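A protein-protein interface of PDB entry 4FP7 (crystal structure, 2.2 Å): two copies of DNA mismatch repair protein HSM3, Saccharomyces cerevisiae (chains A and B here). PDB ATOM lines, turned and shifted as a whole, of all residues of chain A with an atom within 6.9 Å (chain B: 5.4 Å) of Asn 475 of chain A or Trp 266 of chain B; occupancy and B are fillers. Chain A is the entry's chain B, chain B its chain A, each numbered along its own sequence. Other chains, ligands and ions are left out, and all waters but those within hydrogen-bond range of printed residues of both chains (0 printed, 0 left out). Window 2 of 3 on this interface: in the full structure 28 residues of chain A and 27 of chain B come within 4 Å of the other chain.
The backbone NH (N) of Tyr 265 of chain B sits at hydrogen-bond distance from the backbone carbonyl oxygen (O) of Val 474 of chain A (3.1 Å). N of Trp 266 of chain B is in hydrogen-bond range of O of Val 474 of chain A (3.3 Å).
No position is printed for both chains. Of the 8 pairs that touch across the chains among the printed residues, none has its exchanged pair printed and touching as well.
Of chain B, only Tyr 265 and Trp 266 come within 4 Å of Asn 475 of chain A. Of chain A, only Val 474, Asn 475 and Gly 476 come within 4 Å of Trp 266 of chain B. Of the printed residues of chain A, Asp 263 of chain B touches Tyr 470 (3.4 Å) and Val 474 (3.4 Å). Of the printed residues of chain B, Gly 476 of chain A touches Trp 266 (3.9 Å). Of the printed residues of chain B, Tyr 470 of chain A touches Asp 263 (3.4 Å). Printed residues of chain A within 4 Å of Lys 264 of chain B: Val 474. The nearest printed residue of chain B that does not touch Asn 475 of chain A is Asp 263 of chain B (5.5 Å).
Among the printed residues, merely in contact across the chains: Tyr 470 of chain A with Asp 263 of chain B (3.4 Å), Val 474 of chain A with Asp 263 of chain B (3.4 Å), Asn 475 of chain A with Tyr 265 of chain B (3.5 Å), Asn 475 of chain A with Trp 266 of chain B (3.6 Å), Val 474 of chain A with Lys 264 of chain B (3.8 Å) and Gly 476 of chain A with Trp 266 of chain B (3.9 Å).
Printed residues of chain A that touch a printed residue of chain B: Tyr 470, Val 474, Asn 475 and Gly 476. Hydrophobic or aromatic side chains of chain A within 4 Å of the printed part of chain B: Tyr 470 and Val 474. Hydrophobic or aromatic side chains of chain B that line the printed part of chain A: Tyr 265 and Trp 266.
The backbone carbonyl oxygen (O) of Ile 218 of chain B is in hydrogen-bond range of the side-chain amino group (NZ) of Lys 264 of chain B, at 2.9 Å. The side-chain amino group of Lys 264 of chain B is in hydrogen-bond range of the backbone carbonyl oxygen of Phe 215 of chain B (2.9 Å). The side-chain hydroxyl (OH) of Tyr 265 of chain B lies within hydrogen-bond range of the side-chain carboxylate (OD1) of Asp 263 of chain B, at 2.7 Å.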
ATOM      1  N   TYR A 470      26.311  -4.932  34.177  1.00  0.00           N
ATOM      2  CA  TYR A 470      25.689  -6.130  34.705  1.00  0.00           C
ATOM      3  C   TYR A 470      24.949  -6.809  33.572  1.00  0.00           C
ATOM      4  O   TYR A 470      25.109  -8.015  33.371  1.00  0.00           O
ATOM      5  CB  TYR A 470      24.720  -5.835  35.852  1.00  0.00           C
ATOM      6  CG  TYR A 470      24.203  -7.116  36.490  1.00  0.00           C
ATOM      7  CD1 TYR A 470      25.078  -7.984  37.144  1.00  0.00           C
ATOM      8  CD2 TYR A 470      22.855  -7.480  36.414  1.00  0.00           C
ATOM      9  CE1 TYR A 470      24.628  -9.168  37.723  1.00  0.00           C
ATOM     10  CE2 TYR A 470      22.392  -8.670  37.000  1.00  0.00           C
ATOM     11  CZ  TYR A 470      23.289  -9.503  37.649  1.00  0.00           C
ATOM     12  OH  TYR A 470      22.869 -10.671  38.233  1.00  0.00           O
ATOM     13  N   SER A 471      24.151  -6.020  32.841  1.00  0.00           N
ATOM     14  CA  SER A 471      23.439  -6.490  31.655  1.00  0.00           C
ATOM     15  C   SER A 471      24.374  -7.164  30.668  1.00  0.00           C
ATOM     16  O   SER A 471      24.091  -8.267  30.206  1.00  0.00           O
ATOM     17  CB  SER A 471      22.711  -5.343  30.953  1.00  0.00           C
ATOM     18  OG  SER A 471      21.487  -5.066  31.605  1.00  0.00           O
ATOM     19  N   LYS A 472      25.480  -6.512  30.340  1.00  0.00           N
ATOM     20  CA  LYS A 472      26.429  -7.103  29.406  1.00  0.00           C
ATOM     21  C   LYS A 472      26.914  -8.466  29.896  1.00  0.00           C
ATOM     22  O   LYS A 472      27.065  -9.395  29.107  1.00  0.00           O
ATOM     23  CB  LYS A 472      27.653  -6.216  29.208  1.00  0.00           C
ATOM     24  CG  LYS A 472      27.413  -4.921  28.455  1.00  0.00           C
ATOM     25  CD  LYS A 472      28.721  -4.135  28.312  1.00  0.00           C
ATOM     26  CE  LYS A 472      28.477  -2.667  27.976  1.00  0.00           C
ATOM     27  NZ  LYS A 472      29.744  -1.951  27.650  1.00  0.00           N
ATOM     28  N   ALA A 473      27.188  -8.580  31.191  1.00  0.00           N
ATOM     29  CA  ALA A 473      27.859  -9.773  31.708  1.00  0.00           C
ATOM     30  C   ALA A 473      26.869 -10.928  31.839  1.00  0.00           C
ATOM     31  O   ALA A 473      27.226 -12.099  31.764  1.00  0.00           O
ATOM     32  CB  ALA A 473      28.485  -9.477  33.059  1.00  0.00           C
ATOM     33  N   VAL A 474      25.615 -10.562  32.037  1.00  0.00           N
ATOM     34  CA  VAL A 474      24.583 -11.498  32.381  1.00  0.00           C
ATOM     35  C   VAL A 474      23.760 -11.860  31.150  1.00  0.00           C
ATOM     36  O   VAL A 474      23.340 -13.005  31.001  1.00  0.00           O
ATOM     37  CB  VAL A 474      23.709 -10.877  33.466  1.00  0.00           C
ATOM     38  CG1 VAL A 474      22.279 -11.205  33.244  1.00  0.00           C
ATOM     39  CG2 VAL A 474      24.177 -11.349  34.828  1.00  0.00           C
ATOM     40  N   ASN A 475      23.566 -10.888  30.259  1.00  0.00           N
ATOM     41  CA  ASN A 475      22.741 -11.066  29.056  1.00  0.00           C
ATOM     42  C   ASN A 475      23.534 -11.313  27.785  1.00  0.00           C
ATOM     43  O   ASN A 475      22.945 -11.626  26.747  1.00  0.00           O
ATOM     44  CB  ASN A 475      21.852  -9.840  28.811  1.00  0.00           C
ATOM     45  CG  ASN A 475      20.776  -9.680  29.861  1.00  0.00           C
ATOM     46  OD1 ASN A 475      20.427 -10.636  30.557  1.00  0.00           O
ATOM     47  ND2 ASN A 475      20.231  -8.467  29.975  1.00  0.00           N
ATOM     48  N   GLY A 476      24.854 -11.156  27.848  1.00  0.00           N
ATOM     49  CA  GLY A 476      25.700 -11.389  26.683  1.00  0.00           C
ATOM     50  C   GLY A 476      25.572 -10.293  25.636  1.00  0.00           C
ATOM     51  O   GLY A 476      25.502  -9.100  25.957  1.00  0.00           O
ATOM     52  N   PHE B 215      28.294 -27.148  31.969  1.00  0.00           N
ATOM     53  CA  PHE B 215      27.596 -25.881  31.811  1.00  0.00           C
ATOM     54  C   PHE B 215      27.882 -24.892  32.957  1.00  0.00           C
ATOM     55  O   PHE B 215      27.856 -23.687  32.759  1.00  0.00           O
ATOM     56  CB  PHE B 215      26.091 -26.071  31.660  1.00  0.00           C
ATOM     57  CG  PHE B 215      25.388 -24.805  31.323  1.00  0.00           C
ATOM     58  CD1 PHE B 215      25.637 -24.169  30.113  1.00  0.00           C
ATOM     59  CD2 PHE B 215      24.524 -24.214  32.224  1.00  0.00           C
ATOM     60  CE1 PHE B 215      25.013 -22.976  29.798  1.00  0.00           C
ATOM     61  CE2 PHE B 215      23.898 -23.019  31.924  1.00  0.00           C
ATOM     62  CZ  PHE B 215      24.142 -22.396  30.707  1.00  0.00           C
ATOM     63  N   ILE B 218      31.035 -22.874  31.834  1.00  0.00           N
ATOM     64  CA  ILE B 218      31.165 -22.394  30.467  1.00  0.00           C
ATOM     65  C   ILE B 218      30.703 -20.956  30.306  1.00  0.00           C
ATOM     66  O   ILE B 218      29.650 -20.558  30.823  1.00  0.00           O
ATOM     67  CB  ILE B 218      30.388 -23.336  29.505  1.00  0.00           C
ATOM     68  CG1 ILE B 218      31.203 -24.600  29.262  1.00  0.00           C
ATOM     69  CG2 ILE B 218      30.077 -22.667  28.185  1.00  0.00           C
ATOM     70  CD1 ILE B 218      32.501 -24.383  28.508  1.00  0.00           C
ATOM     71  N   SER B 219      31.500 -20.179  29.573  1.00  0.00           N
ATOM     72  CA  SER B 219      31.190 -18.769  29.299  1.00  0.00           C
ATOM     73  C   SER B 219      30.420 -18.642  28.005  1.00  0.00           C
ATOM     74  O   SER B 219      30.425 -19.554  27.171  1.00  0.00           O
ATOM     75  CB  SER B 219      32.480 -17.951  29.191  1.00  0.00           C
ATOM     76  OG  SER B 219      33.184 -18.278  28.000  1.00  0.00           O
ATOM     77  N   GLY B 220      29.765 -17.508  27.813  1.00  0.00           N
ATOM     78  CA  GLY B 220      29.095 -17.260  26.545  1.00  0.00           C
ATOM     79  C   GLY B 220      29.934 -17.558  25.303  1.00  0.00           C
ATOM     80  O   GLY B 220      29.444 -18.174  24.354  1.00  0.00           O
ATOM     81  N   PHE B 223      30.479 -21.190  24.514  1.00  0.00           N
ATOM     82  CA  PHE B 223      29.262 -21.998  24.370  1.00  0.00           C
ATOM     83  C   PHE B 223      29.046 -22.477  22.933  1.00  0.00           C
ATOM     84  O   PHE B 223      29.050 -21.681  21.991  1.00  0.00           O
ATOM     85  CB  PHE B 223      28.030 -21.221  24.869  1.00  0.00           C
ATOM     86  CG  PHE B 223      26.785 -22.068  24.984  1.00  0.00           C
ATOM     87  CD1 PHE B 223      26.541 -22.828  26.133  1.00  0.00           C
ATOM     88  CD2 PHE B 223      25.863 -22.117  23.941  1.00  0.00           C
ATOM     89  CE1 PHE B 223      25.390 -23.616  26.238  1.00  0.00           C
ATOM     90  CE2 PHE B 223      24.709 -22.911  24.036  1.00  0.00           C
ATOM     91  CZ  PHE B 223      24.479 -23.661  25.189  1.00  0.00           C
ATOM     92  N   ASP B 263      22.883 -16.622  36.772  1.00  0.00           N
ATOM     93  CA  ASP B 263      22.583 -15.503  35.864  1.00  0.00           C
ATOM     94  C   ASP B 263      23.316 -15.598  34.531  1.00  0.00           C
ATOM     95  O   ASP B 263      24.140 -14.740  34.211  1.00  0.00           O
ATOM     96  CB  ASP B 263      22.905 -14.168  36.539  1.00  0.00           C
ATOM     97  CG  ASP B 263      22.166 -14.002  37.850  1.00  0.00           C
ATOM     98  OD1 ASP B 263      20.946 -13.709  37.806  1.00  0.00           O
ATOM     99  OD2 ASP B 263      22.799 -14.186  38.916  1.00  0.00           O
ATOM    100  N   LYS B 264      23.031 -16.659  33.774  1.00  0.00           N
ATOM    101  CA  LYS B 264      23.607 -16.839  32.443  1.00  0.00           C
ATOM    102  C   LYS B 264      22.497 -16.724  31.426  1.00  0.00           C
ATOM    103  O   LYS B 264      22.299 -17.600  30.588  1.00  0.00           O
ATOM    104  CB  LYS B 264      24.289 -18.192  32.321  1.00  0.00           C
ATOM    105  CG  LYS B 264      25.399 -18.397  33.310  1.00  0.00           C
ATOM    106  CD  LYS B 264      26.086 -19.739  33.100  1.00  0.00           C
ATOM    107  CE  LYS B 264      27.450 -19.723  33.768  1.00  0.00           C
ATOM    108  NZ  LYS B 264      28.318 -20.841  33.335  1.00  0.00           N
ATOM    109  N   TYR B 265      21.769 -15.623  31.514  1.00  0.00           N
ATOM    110  CA  TYR B 265      20.626 -15.375  30.659  1.00  0.00           C
ATOM    111  C   TYR B 265      20.975 -15.397  29.168  1.00  0.00           C
ATOM    112  O   TYR B 265      20.091 -15.641  28.335  1.00  0.00           O
ATOM    113  CB  TYR B 265      19.937 -14.071  31.098  1.00  0.00           C
ATOM    114  CG  TYR B 265      19.573 -14.126  32.580  1.00  0.00           C
ATOM    115  CD1 TYR B 265      18.937 -15.247  33.114  1.00  0.00           C
ATOM    116  CD2 TYR B 265      19.902 -13.091  33.450  1.00  0.00           C
ATOM    117  CE1 TYR B 265      18.632 -15.326  34.459  1.00  0.00           C
ATOM    118  CE2 TYR B 265      19.591 -13.158  34.812  1.00  0.00           C
ATOM    119  CZ  TYR B 265      18.959 -14.281  35.308  1.00  0.00           C
ATOM    120  OH  TYR B 265      18.642 -14.383  36.651  1.00  0.00           O
ATOM    121  N   TRP B 266      22.249 -15.176  28.829  1.00  0.00           N
ATOM    122  CA  TRP B 266      22.680 -15.255  27.426  1.00  0.00           C
ATOM    123  C   TRP B 266      22.409 -16.629  26.845  1.00  0.00           C
ATOM    124  O   TRP B 266      22.140 -16.758  25.659  1.00  0.00           O
ATOM    125  CB  TRP B 266      24.159 -14.947  27.274  1.00  0.00           C
ATOM    126  CG  TRP B 266      25.044 -15.738  28.159  1.00  0.00           C
ATOM    127  CD1 TRP B 266      25.577 -15.330  29.341  1.00  0.00           C
ATOM    128  CD2 TRP B 266      25.530 -17.070  27.935  1.00  0.00           C
ATOM    129  NE1 TRP B 266      26.358 -16.327  29.878  1.00  0.00           N
ATOM    130  CE2 TRP B 266      26.342 -17.407  29.038  1.00  0.00           C
ATOM    131  CE3 TRP B 266      25.354 -18.008  26.918  1.00  0.00           C
ATOM    132  CZ2 TRP B 266      26.988 -18.637  29.149  1.00  0.00           C
ATOM    133  CZ3 TRP B 266      25.988 -19.248  27.038  1.00  0.00           C
ATOM    134  CH2 TRP B 266      26.799 -19.542  28.139  1.00  0.00           C
ATOM    135  N   ALA B 267      22.457 -17.658  27.687  1.00  0.00           N
ATOM    136  CA  ALA B 267      22.146 -19.001  27.233  1.00  0.00           C
ATOM    137  C   ALA B 267      20.677 -19.162  26.790  1.00  0.00           C
ATOM    138  O   ALA B 267      20.378 -20.046  25.987  1.00  0.00           O
ATOM    139  CB  ALA B 267      22.492 -20.010  28.295  1.00  0.00           C
ATOM    140  N   LEU B 268      19.764 -18.322  27.284  1.00  0.00           N
ATOM    141  CA  LEU B 268      18.346 -18.532  26.974  1.00  0.00           C
ATOM    142  C   LEU B 268      18.046 -18.549  25.474  1.00  0.00           C
ATOM    143  O   LEU B 268      17.219 -19.353  25.008  1.00  0.00           O
ATOM    144  CB  LEU B 268      17.447 -17.509  27.669  1.00  0.00           C
ATOM    145  CG  LEU B 268      17.207 -17.780  29.158  1.00  0.00           C
ATOM    146  CD1 LEU B 268      16.480 -16.594  29.762  1.00  0.00           C
ATOM    147  CD2 LEU B 268      16.410 -19.079  29.383  1.00  0.00           C
ATOM    148  N   ARG B 269      18.690 -17.664  24.720  1.00  0.00           N
ATOM    149  CA  ARG B 269      18.406 -17.548  23.279  1.00  0.00           C
ATOM    150  C   ARG B 269      18.730 -18.860  22.564  1.00  0.00           C
ATOM    151  O   ARG B 269      18.147 -19.175  21.539  1.00  0.00           O
ATOM    152  CB  ARG B 269      19.199 -16.398  22.642  1.00  0.00           C
ATOM    153  N   HIS B 270      19.658 -19.628  23.132  1.00  0.00           N
ATOM    154  CA  HIS B 270      20.057 -20.912  22.560  1.00  0.00           C
ATOM    155  C   HIS B 270      19.104 -22.065  22.877  1.00  0.00           C
ATOM    156  O   HIS B 270      19.210 -23.124  22.283  1.00  0.00           O
ATOM    157  CB  HIS B 270      21.445 -21.273  23.062  1.00  0.00           C
ATOM    158  CG  HIS B 270      22.504 -20.294  22.662  1.00  0.00           C
ATOM    159  ND1 HIS B 270      22.991 -20.210  21.375  1.00  0.00           N
ATOM    160  CD2 HIS B 270      23.171 -19.357  23.377  1.00  0.00           C
ATOM    161  CE1 HIS B 270      23.913 -19.267  21.314  1.00  0.00           C
ATOM    162  NE2 HIS B 270      24.046 -18.737  22.517  1.00  0.00           N
